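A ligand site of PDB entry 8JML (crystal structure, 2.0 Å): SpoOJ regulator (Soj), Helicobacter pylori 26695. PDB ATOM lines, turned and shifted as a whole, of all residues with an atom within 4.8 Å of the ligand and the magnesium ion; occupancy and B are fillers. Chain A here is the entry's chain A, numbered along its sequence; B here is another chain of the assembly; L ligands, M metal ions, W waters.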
ATOM      1  N   LYS A  12       7.992 -18.851  -3.306  1.00  0.00           N
ATOM      2  CA  LYS A  12       8.613 -18.838  -1.985  1.00  0.00           C
ATOM      3  C   LYS A  12       8.390 -17.463  -1.373  1.00  0.00           C
ATOM      4  O   LYS A  12       8.508 -16.430  -2.034  1.00  0.00           O
ATOM      5  CB  LYS A  12      10.125 -19.122  -2.045  1.00  0.00           C
ATOM      6  CG  LYS A  12      10.797 -19.311  -0.670  1.00  0.00           C
ATOM      7  CD  LYS A  12      10.366 -20.597   0.040  1.00  0.00           C
ATOM      8  CE  LYS A  12      11.102 -20.758   1.370  1.00  0.00           C
ATOM      9  NZ  LYS A  12      10.651 -19.786   2.387  1.00  0.00           N
ATOM     10  N   GLY A  13       8.056 -17.428  -0.100  1.00  0.00           N
ATOM     11  CA  GLY A  13       7.874 -16.136   0.491  1.00  0.00           C
ATOM     12  C   GLY A  13       9.156 -15.446   0.902  1.00  0.00           C
ATOM     13  O   GLY A  13      10.121 -16.115   1.278  1.00  0.00           O
ATOM     14  N   GLY A  14       9.172 -14.114   0.797  1.00  0.00           N
ATOM     15  CA  GLY A  14      10.230 -13.300   1.369  1.00  0.00           C
ATOM     16  C   GLY A  14      11.565 -13.420   0.697  1.00  0.00           C
ATOM     17  O   GLY A  14      12.612 -13.348   1.359  1.00  0.00           O
ATOM     18  N   VAL A  15      11.549 -13.632  -0.610  1.00  0.00           N
ATOM     19  CA  VAL A  15      12.789 -13.776  -1.366  1.00  0.00           C
ATOM     20  C   VAL A  15      13.205 -12.508  -2.094  1.00  0.00           C
ATOM     21  O   VAL A  15      14.131 -12.535  -2.894  1.00  0.00           O
ATOM     22  CB  VAL A  15      12.733 -14.939  -2.351  1.00  0.00           C
ATOM     23  CG1 VAL A  15      12.596 -16.246  -1.573  1.00  0.00           C
ATOM     24  CG2 VAL A  15      11.573 -14.749  -3.328  1.00  0.00           C
ATOM     25  N   GLY A  16      12.483 -11.417  -1.866  1.00  0.00           N
ATOM     26  CA  GLY A  16      12.846 -10.145  -2.449  1.00  0.00           C
ATOM     27  C   GLY A  16      12.103  -9.744  -3.703  1.00  0.00           C
ATOM     28  O   GLY A  16      12.620  -8.908  -4.426  1.00  0.00           O
ATOM     29  N   LYS A  17      10.935 -10.338  -3.971  1.00  0.00           N
ATOM     30  CA  LYS A  17      10.097  -9.979  -5.125  1.00  0.00           C
ATOM     31  C   LYS A  17       9.709  -8.505  -5.153  1.00  0.00           C
ATOM     32  O   LYS A  17       9.897  -7.827  -6.179  1.00  0.00           O
ATOM     33  CB  LYS A  17       8.793 -10.791  -5.128  1.00  0.00           C
ATOM     34  CG  LYS A  17       8.949 -12.298  -5.314  1.00  0.00           C
ATOM     35  CD  LYS A  17       7.584 -12.995  -5.305  1.00  0.00           C
ATOM     36  CE  LYS A  17       6.896 -12.972  -3.936  1.00  0.00           C
ATOM     37  NZ  LYS A  17       7.646 -13.694  -2.859  1.00  0.00           N
ATOM     38  N   THR A  18       9.219  -8.017  -4.012  1.00  0.00           N
ATOM     39  CA  THR A  18       8.795  -6.634  -3.875  1.00  0.00           C
ATOM     40  C   THR A  18       9.954  -5.656  -3.958  1.00  0.00           C
ATOM     41  O   THR A  18       9.870  -4.664  -4.682  1.00  0.00           O
ATOM     42  CB  THR A  18       8.005  -6.434  -2.564  1.00  0.00           C
ATOM     43  OG1 THR A  18       6.794  -7.193  -2.665  1.00  0.00           O
ATOM     44  CG2 THR A  18       7.662  -4.978  -2.295  1.00  0.00           C
ATOM     45  N   THR A  19      11.048  -5.975  -3.271  1.00  0.00           N
ATOM     46  CA  THR A  19      12.284  -5.184  -3.308  1.00  0.00           C
ATOM     47  C   THR A  19      12.841  -5.079  -4.720  1.00  0.00           C
ATOM     48  O   THR A  19      13.207  -3.991  -5.171  1.00  0.00           O
ATOM     49  CB  THR A  19      13.332  -5.774  -2.349  1.00  0.00           C
ATOM     50  OG1 THR A  19      12.777  -5.805  -1.035  1.00  0.00           O
ATOM     51  CG2 THR A  19      14.615  -4.947  -2.335  1.00  0.00           C
ATOM     52  N   ASN A  45       2.800  -4.593  -0.334  1.00  0.00           N
ATOM     53  CA  ASN A  45       4.086  -4.095   0.153  1.00  0.00           C
ATOM     54  C   ASN A  45       4.767  -3.127  -0.805  1.00  0.00           C
ATOM     55  O   ASN A  45       5.513  -2.238  -0.373  1.00  0.00           O
ATOM     56  CB  ASN A  45       5.025  -5.253   0.492  1.00  0.00           C
ATOM     57  CG  ASN A  45       4.547  -6.091   1.671  1.00  0.00           C
ATOM     58  OD1 ASN A  45       4.948  -7.249   1.812  1.00  0.00           O
ATOM     59  ND2 ASN A  45       3.703  -5.518   2.515  1.00  0.00           N
ATOM     60  N   ASP A 130       4.550  -6.936  -9.564  1.00  0.00           N
ATOM     61  CA  ASP A 130       5.006  -7.592  -8.339  1.00  0.00           C
ATOM     62  C   ASP A 130       3.988  -8.653  -7.890  1.00  0.00           C
ATOM     63  O   ASP A 130       2.913  -8.305  -7.467  1.00  0.00           O
ATOM     64  CB  ASP A 130       5.157  -6.524  -7.246  1.00  0.00           C
ATOM     65  CG  ASP A 130       5.690  -7.075  -5.937  1.00  0.00           C
ATOM     66  OD1 ASP A 130       6.357  -8.135  -5.960  1.00  0.00           O
ATOM     67  OD2 ASP A 130       5.445  -6.438  -4.877  1.00  0.00           O
ATOM     68  N   SER A 131       4.368  -9.935  -7.948  1.00  0.00           N
ATOM     69  CA  SER A 131       3.456 -11.074  -7.656  1.00  0.00           C
ATOM     70  C   SER A 131       3.472 -11.505  -6.182  1.00  0.00           C
ATOM     71  O   SER A 131       4.487 -11.296  -5.505  1.00  0.00           O
ATOM     72  CB  SER A 131       3.882 -12.277  -8.525  1.00  0.00           C
ATOM     73  OG  SER A 131       3.758 -11.983  -9.899  1.00  0.00           O
ATOM     74  N   PRO A 133       3.483 -14.483  -2.992  1.00  0.00           N
ATOM     75  CA  PRO A 133       4.129 -15.800  -2.840  1.00  0.00           C
ATOM     76  C   PRO A 133       3.183 -17.014  -2.976  1.00  0.00           C
ATOM     77  O   PRO A 133       2.949 -17.727  -2.002  1.00  0.00           O
ATOM     78  CB  PRO A 133       4.691 -15.734  -1.419  1.00  0.00           C
ATOM     79  CG  PRO A 133       3.809 -14.755  -0.711  1.00  0.00           C
ATOM     80  CD  PRO A 133       3.541 -13.710  -1.732  1.00  0.00           C
ATOM     81  N   MET A 190      19.547 -11.055  -1.567  1.00  0.00           N
ATOM     82  CA  MET A 190      20.039 -11.177  -0.169  1.00  0.00           C
ATOM     83  C   MET A 190      21.321 -11.997  -0.065  1.00  0.00           C
ATOM     84  O   MET A 190      21.508 -12.783   0.858  1.00  0.00           O
ATOM     85  CB  MET A 190      18.955 -11.742   0.755  1.00  0.00           C
ATOM     86  CG  MET A 190      17.789 -10.823   0.826  1.00  0.00           C
ATOM     87  SD  MET A 190      16.372 -11.435   1.743  1.00  0.00           S
ATOM     88  CE  MET A 190      15.728 -12.471   0.471  1.00  0.00           C
ATOM     89  N   ILE A 225      22.061  -9.498  -6.048  1.00  0.00           N
ATOM     90  CA  ILE A 225      21.763  -8.379  -5.150  1.00  0.00           C
ATOM     91  C   ILE A 225      22.302  -8.755  -3.792  1.00  0.00           C
ATOM     92  O   ILE A 225      21.862  -9.758  -3.208  1.00  0.00           O
ATOM     93  CB  ILE A 225      20.251  -8.097  -5.035  1.00  0.00           C
ATOM     94  CG1 ILE A 225      19.574  -8.029  -6.428  1.00  0.00           C
ATOM     95  CG2 ILE A 225      20.017  -6.827  -4.227  1.00  0.00           C
ATOM     96  CD1 ILE A 225      20.146  -6.987  -7.405  1.00  0.00           C
ATOM     97  N   PRO A 226      23.273  -7.983  -3.267  1.00  0.00           N
ATOM     98  CA  PRO A 226      23.857  -8.310  -1.965  1.00  0.00           C
ATOM     99  C   PRO A 226      22.872  -8.067  -0.817  1.00  0.00           C
ATOM    100  O   PRO A 226      21.922  -7.268  -0.979  1.00  0.00           O
ATOM    101  CB  PRO A 226      25.026  -7.332  -1.854  1.00  0.00           C
ATOM    102  CG  PRO A 226      24.576  -6.131  -2.650  1.00  0.00           C
ATOM    103  CD  PRO A 226      23.775  -6.696  -3.798  1.00  0.00           C
ATOM    104  N   LYS A 227      23.073  -8.778   0.289  1.00  0.00           N
ATOM    105  CA  LYS A 227      22.360  -8.479   1.516  1.00  0.00           C
ATOM    106  C   LYS A 227      22.814  -7.115   1.978  1.00  0.00           C
ATOM    107  O   LYS A 227      24.023  -6.855   2.095  1.00  0.00           O
ATOM    108  CB  LYS A 227      22.668  -9.511   2.589  1.00  0.00           C
ATOM    109  CG  LYS A 227      21.860  -9.258   3.882  1.00  0.00           C
ATOM    110  CD  LYS A 227      21.852 -10.475   4.785  1.00  0.00           C
ATOM    111  CE  LYS A 227      21.069 -10.197   6.071  1.00  0.00           C
ATOM    112  NZ  LYS A 227      19.600  -9.971   5.850  1.00  0.00           N
ATOM    113  N   SER A 228      21.856  -6.220   2.176  1.00  0.00           N
ATOM    114  CA  SER A 228      22.196  -4.843   2.468  1.00  0.00           C
ATOM    115  C   SER A 228      21.250  -4.247   3.482  1.00  0.00           C
ATOM    116  O   SER A 228      20.044  -4.214   3.247  1.00  0.00           O
ATOM    117  CB  SER A 228      22.129  -4.015   1.181  1.00  0.00           C
ATOM    118  OG  SER A 228      22.233  -2.638   1.487  1.00  0.00           O
ATOM    119  N   LEU A 231      18.997  -1.506   2.024  1.00  0.00           N
ATOM    120  CA  LEU A 231      17.935  -2.001   1.165  1.00  0.00           C
ATOM    121  C   LEU A 231      16.697  -2.334   1.985  1.00  0.00           C
ATOM    122  O   LEU A 231      15.558  -2.097   1.556  1.00  0.00           O
ATOM    123  CB  LEU A 231      18.434  -3.260   0.453  1.00  0.00           C
ATOM    124  CG  LEU A 231      18.066  -3.591  -0.974  1.00  0.00           C
ATOM    125  CD1 LEU A 231      17.987  -2.382  -1.796  1.00  0.00           C
ATOM    126  CD2 LEU A 231      19.155  -4.410  -1.547  1.00  0.00           C
ATOM    127  N   ALA A 232      16.916  -2.856   3.180  1.00  0.00           N
ATOM    128  CA  ALA A 232      15.823  -3.183   4.092  1.00  0.00           C
ATOM    129  C   ALA A 232      15.256  -1.904   4.726  1.00  0.00           C
ATOM    130  O   ALA A 232      14.048  -1.828   5.006  1.00  0.00           O
ATOM    131  CB  ALA A 232      16.317  -4.152   5.172  1.00  0.00           C
ATOM    132  N   PRO A 235      12.340   0.908   2.298  1.00  0.00           N
ATOM    133  CA  PRO A 235      10.862   1.061   2.267  1.00  0.00           C
ATOM    134  C   PRO A 235      10.260   1.742   3.499  1.00  0.00           C
ATOM    135  O   PRO A 235       9.169   2.290   3.377  1.00  0.00           O
ATOM    136  CB  PRO A 235      10.355  -0.390   2.177  1.00  0.00           C
ATOM    137  CG  PRO A 235      11.491  -1.249   2.668  1.00  0.00           C
ATOM    138  CD  PRO A 235      12.708  -0.528   2.187  1.00  0.00           C
ATOM    139  N   LYS B  12       2.938 -12.606   5.807  1.00  0.00           N
ATOM    140  CA  LYS B  12       4.173 -12.141   5.186  1.00  0.00           C
ATOM    141  C   LYS B  12       5.030 -13.342   4.826  1.00  0.00           C
ATOM    142  O   LYS B  12       5.112 -14.329   5.574  1.00  0.00           O
ATOM    143  CB  LYS B  12       4.951 -11.214   6.129  1.00  0.00           C
ATOM    144  CG  LYS B  12       6.207 -10.539   5.502  1.00  0.00           C
ATOM    145  CD  LYS B  12       5.849  -9.543   4.423  1.00  0.00           C
ATOM    146  CE  LYS B  12       7.089  -8.934   3.803  1.00  0.00           C
ATOM    147  NZ  LYS B  12       7.908  -9.919   3.044  1.00  0.00           N
ATOM    148  N   GLY B  13       5.649 -13.283   3.655  1.00  0.00           N
ATOM    149  CA  GLY B  13       6.493 -14.376   3.263  1.00  0.00           C
ATOM    150  C   GLY B  13       7.880 -14.380   3.887  1.00  0.00           C
ATOM    151  O   GLY B  13       8.465 -13.344   4.127  1.00  0.00           O
ATOM    152  N   GLN B 154       9.454 -11.307  11.741  1.00  0.00           N
ATOM    153  CA  GLN B 154      10.763 -10.834  11.311  1.00  0.00           C
ATOM    154  C   GLN B 154      10.736  -9.326  11.518  1.00  0.00           C
ATOM    155  O   GLN B 154       9.830  -8.645  11.020  1.00  0.00           O
ATOM    156  CB  GLN B 154      10.937 -11.182   9.833  1.00  0.00           C
ATOM    157  CG  GLN B 154      12.213 -10.687   9.190  1.00  0.00           C
ATOM    158  CD  GLN B 154      12.162 -10.883   7.692  1.00  0.00           C
ATOM    159  OE1 GLN B 154      11.145 -10.594   7.044  1.00  0.00           O
ATOM    160  NE2 GLN B 154      13.236 -11.415   7.119  1.00  0.00           N
ATOM    161  N   GLU B 156      11.430  -6.249  10.432  1.00  0.00           N
ATOM    162  CA  GLU B 156      11.805  -5.417   9.319  1.00  0.00           C
ATOM    163  C   GLU B 156      10.512  -4.692   9.027  1.00  0.00           C
ATOM    164  O   GLU B 156       9.527  -4.939   9.730  1.00  0.00           O
ATOM    165  CB  GLU B 156      12.346  -6.264   8.151  1.00  0.00           C
ATOM    166  CG  GLU B 156      13.798  -6.692   8.390  1.00  0.00           C
ATOM    167  CD  GLU B 156      14.391  -7.524   7.280  1.00  0.00           C
ATOM    168  OE1 GLU B 156      13.760  -7.592   6.208  1.00  0.00           O
ATOM    169  OE2 GLU B 156      15.471  -8.122   7.486  1.00  0.00           O
ATOM    170  N   PHE B 157      10.509  -3.799   8.043  1.00  0.00           N
ATOM    171  CA  PHE B 157       9.510  -2.728   7.980  1.00  0.00           C
ATOM    172  C   PHE B 157       8.063  -3.176   7.746  1.00  0.00           C
ATOM    173  O   PHE B 157       7.139  -2.661   8.385  1.00  0.00           O
ATOM    174  CB  PHE B 157       9.887  -1.664   6.937  1.00  0.00           C
ATOM    175  CG  PHE B 157       8.779  -0.684   6.663  1.00  0.00           C
ATOM    176  CD1 PHE B 157       8.361   0.218   7.644  1.00  0.00           C
ATOM    177  CD2 PHE B 157       8.119  -0.691   5.437  1.00  0.00           C
ATOM    178  CE1 PHE B 157       7.328   1.108   7.400  1.00  0.00           C
ATOM    179  CE2 PHE B 157       7.092   0.192   5.179  1.00  0.00           C
ATOM    180  CZ  PHE B 157       6.695   1.106   6.163  1.00  0.00           C
ATOM    181  N   PHE B 158       7.872  -4.177   6.891  1.00  0.00           N
ATOM    182  CA  PHE B 158       6.520  -4.634   6.560  1.00  0.00           C
ATOM    183  C   PHE B 158       5.788  -5.380   7.699  1.00  0.00           C
ATOM    184  O   PHE B 158       4.587  -5.616   7.615  1.00  0.00           O
ATOM    185  CB  PHE B 158       6.519  -5.468   5.276  1.00  0.00           C
ATOM    186  CG  PHE B 158       7.127  -4.762   4.107  1.00  0.00           C
ATOM    187  CD1 PHE B 158       6.621  -3.534   3.682  1.00  0.00           C
ATOM    188  CD2 PHE B 158       8.200  -5.319   3.409  1.00  0.00           C
ATOM    189  CE1 PHE B 158       7.185  -2.858   2.582  1.00  0.00           C
ATOM    190  CE2 PHE B 158       8.771  -4.664   2.313  1.00  0.00           C
ATOM    191  CZ  PHE B 158       8.262  -3.431   1.912  1.00  0.00           C
HETATM  192  P1  LIG L   1       6.506 -11.683   0.071  1.00  0.00           P
HETATM  193  O1  LIG L   1       5.808 -10.893  -1.006  1.00  0.00           O
HETATM  194  O2  LIG L   1       6.034 -11.458   1.480  1.00  0.00           O
HETATM  195  O3  LIG L   1       6.674 -13.132  -0.331  1.00  0.00           O
HETATM  196  P2  LIG L   1       8.925 -10.704  -1.139  1.00  0.00           P
HETATM  197  O4  LIG L   1       8.238  -9.624  -1.930  1.00  0.00           O
HETATM  198  O5  LIG L   1       9.378 -11.920  -1.889  1.00  0.00           O
HETATM  199  O6  LIG L   1       8.023 -11.116   0.129  1.00  0.00           O
HETATM  200  P3  LIG L   1      10.457  -8.644   0.163  1.00  0.00           P
HETATM  201  O7  LIG L   1      10.860  -7.737  -0.950  1.00  0.00           O
HETATM  202  O8  LIG L   1       9.283  -8.210   1.039  1.00  0.00           O
HETATM  203  O9  LIG L   1      10.228 -10.134  -0.405  1.00  0.00           O
HETATM  204  O10 LIG L   1      11.764  -8.934   1.017  1.00  0.00           O
HETATM  205  C1  LIG L   1      11.763  -9.626   2.257  1.00  0.00           C
HETATM  206  C2  LIG L   1      12.408  -8.754   3.336  1.00  0.00           C
HETATM  207  O11 LIG L   1      13.823  -8.641   3.153  1.00  0.00           O
HETATM  208  C3  LIG L   1      11.876  -7.327   3.307  1.00  0.00           C
HETATM  209  O12 LIG L   1      11.690  -6.943   4.663  1.00  0.00           O
HETATM  210  C4  LIG L   1      12.970  -6.464   2.671  1.00  0.00           C
HETATM  211  O13 LIG L   1      12.995  -5.137   3.168  1.00  0.00           O
HETATM  212  C5  LIG L   1      14.221  -7.265   2.957  1.00  0.00           C
HETATM  213  N1  LIG L   1      15.170  -7.351   1.829  1.00  0.00           N
HETATM  214  C6  LIG L   1      14.907  -7.625   0.530  1.00  0.00           C
HETATM  215  N2  LIG L   1      16.063  -7.687  -0.176  1.00  0.00           N
HETATM  216  C7  LIG L   1      17.076  -7.435   0.685  1.00  0.00           C
HETATM  217  C8  LIG L   1      18.546  -7.371   0.613  1.00  0.00           C
HETATM  218  N3  LIG L   1      19.192  -7.584  -0.571  1.00  0.00           N
HETATM  219  N4  LIG L   1      19.211  -7.119   1.756  1.00  0.00           N
HETATM  220  C9  LIG L   1      18.585  -6.964   2.933  1.00  0.00           C
HETATM  221  N5  LIG L   1      17.255  -7.010   3.091  1.00  0.00           N
HETATM  222  C10 LIG L   1      16.480  -7.247   2.009  1.00  0.00           C
HETATM  223 MG    MG M   1       6.303  -9.034  -1.757  1.00  0.00          MG
HETATM  224  O   HOH W   1      15.364 -10.075   4.893  1.00  0.00           O
HETATM  225  O   HOH W   2      12.283  -3.822   5.743  1.00  0.00           O
HETATM  226  O   HOH W   3       9.925 -11.197   4.517  1.00  0.00           O
HETATM  227  O   HOH W   4       6.727  -8.094   0.122  1.00  0.00           O
HETATM  228  O   HOH W   5       3.908  -9.731   1.726  1.00  0.00           O
HETATM  229  O   HOH W   6      17.260  -7.894   5.739  1.00  0.00           O
HETATM  230  O   HOH W   7       4.326  -8.267  -1.516  1.00  0.00           O
HETATM  231  O   HOH W   8       9.690  -6.902   6.237  1.00  0.00           O
HETATM  232  O   HOH W   9      17.076  -8.008  -2.892  1.00  0.00           O
HETATM  233  O   HOH W  10       3.074 -10.440  -1.151  1.00  0.00           O
HETATM  234  O   HOH W  11       5.806  -9.586  -3.706  1.00  0.00           O
HETATM  235  O   HOH W  12      12.718  -3.720   0.714  1.00  0.00           O
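The backbone NH of Thr 18 is in hydrogen-bond range of an oxygen (O7) of the ligand (3.5 Å).
O5 of the ligand sits at hydrogen-bond distance from N of Lys 17 (3.0 Å).
The side-chain amino group of Lys 17 is in salt-bridge range of an oxygen (O5) of the ligand (2.7 Å).
An oxygen (O12) of the ligand sits at hydrogen-bond distance from the side-chain carboxylate of Glu 156 of chain B.
An oxygen (O7) of the ligand sits at hydrogen-bond distance from the backbone NH (N) of Thr 19.
The side-chain hydroxyl (OG1) of Thr 19 sits at hydrogen-bond distance from an oxygen (O7) of the ligand (2.7 Å).
The backbone carbonyl oxygen of Pro 226 is in hydrogen-bond range of a nitrogen (N3) of the ligand, at 2.8 Å.
The backbone NH (N) of Ser 228 sits at hydrogen-bond distance from a nitrogen (N4) of the ligand, at 2.8 Å.
N of Gly 13 of chain B sits at hydrogen-bond distance from O2 of the ligand, 2.9 Å away.
An oxygen (O2) of the ligand lies within salt-bridge range of the side-chain amino group (NZ) of Lys 12 of chain B, 2.9 Å away.
An oxygen (O3) of the ligand is in hydrogen-bond range of the backbone NH (N) of Gly 14 (2.9 Å).
N of Gly 16 is in hydrogen-bond range of O9 of the ligand.
The backbone NH of Val 15 lies within hydrogen-bond range of an oxygen (O5) of the ligand (3.0 Å).
CA of Gly 13 of chain A touches O3 of the ligand, 3.3 Å away.
CG of Pro 133 touches O3 of the ligand (3.3 Å).
CG of Met 190 touches C7 of the ligand (3.5 Å).
Ile 225 touches the ligand (CG2 to N3, 3.8 Å).
CA of Lys 227 touches N4 of the ligand, at 3.4 Å.
Leu 231 touches the ligand.
Ala 232 touches the ligand (CA to O13, 3.6 Å).
CE2 of Phe 158 of chain B touches O8 of the ligand, 3.8 Å away.
Hydrophobic or aromatic side chains that line the ligand: Val 15, Pro 133, Met 190, Ile 225, Leu 231, Ala 232 and Phe 158 of chain B.
Within 4 Å of the ligand: Gly 13 of chain A, Gly 14, Val 15, Gly 16, Lys 17, Thr 18, Thr 19, Pro 133, Met 190, Ile 225, Pro 226, Lys 227, Ser 228, Leu 231, Ala 232, Lys 12 of chain B, Gly 13 of chain B, Glu 156 of chain B and Phe 158 of chain B.
The side-chain carboxylate (OD1) of Asp 130 lies within hydrogen-bond range of the backbone NH (N) of Thr 18 (3.5 Å).
O of Lys 12 of chain A sits at hydrogen-bond distance from NZ of Lys 17 (3.0 Å).
N of Leu 231 is in hydrogen-bond range of OG of Ser 228, at 3.5 Å.
N of Gly 14 sits close to O of Gly 13 of chain B, 3.5 Å away.
The backbone NH (N) of Met 190 sits at hydrogen-bond distance from the backbone carbonyl oxygen (O) of Ile 225 (3.1 Å).
Water W11 bridges the side-chain carboxylate (OD1) of Asp 130 and the backbone carbonyl oxygen (O) of Ser 131.
Water W4 lies within hydrogen-bond range of the side-chain amide oxygen (OD1) of Asn 45 (2.6 Å) and an oxygen (O8) of the ligand (2.7 Å).
Water W8 bridges O12 of the ligand (2.5 Å) and N of Phe 158 of chain B (3.3 Å).
Water W5 lies within hydrogen-bond range of OD1 of Asn 45 (2.7 Å) and O2 of the ligand (2.8 Å).
Water W12 lies within hydrogen-bond range of OG1 of Thr 19 (2.7 Å), O13 of the ligand (2.8 Å) and O of Leu 231 (3.4 Å).
Water W2 lies within hydrogen-bond range of O of Ala 232, N of Phe 157 of chain B and O13 of the ligand.
O4 of the ligand is bound to the magnesium ion (2.0 Å).
The magnesium ion is bound by O1 of the ligand, 2.1 Å away.
Water W11 is bound to the magnesium ion, at 2.1 Å.
The magnesium ion is bound by OG1 of Thr 18, at 2.1 Å.
Water W7 is bound to the magnesium ion (2.1 Å).
The magnesium ion is bound by water W4, 2.1 Å away.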
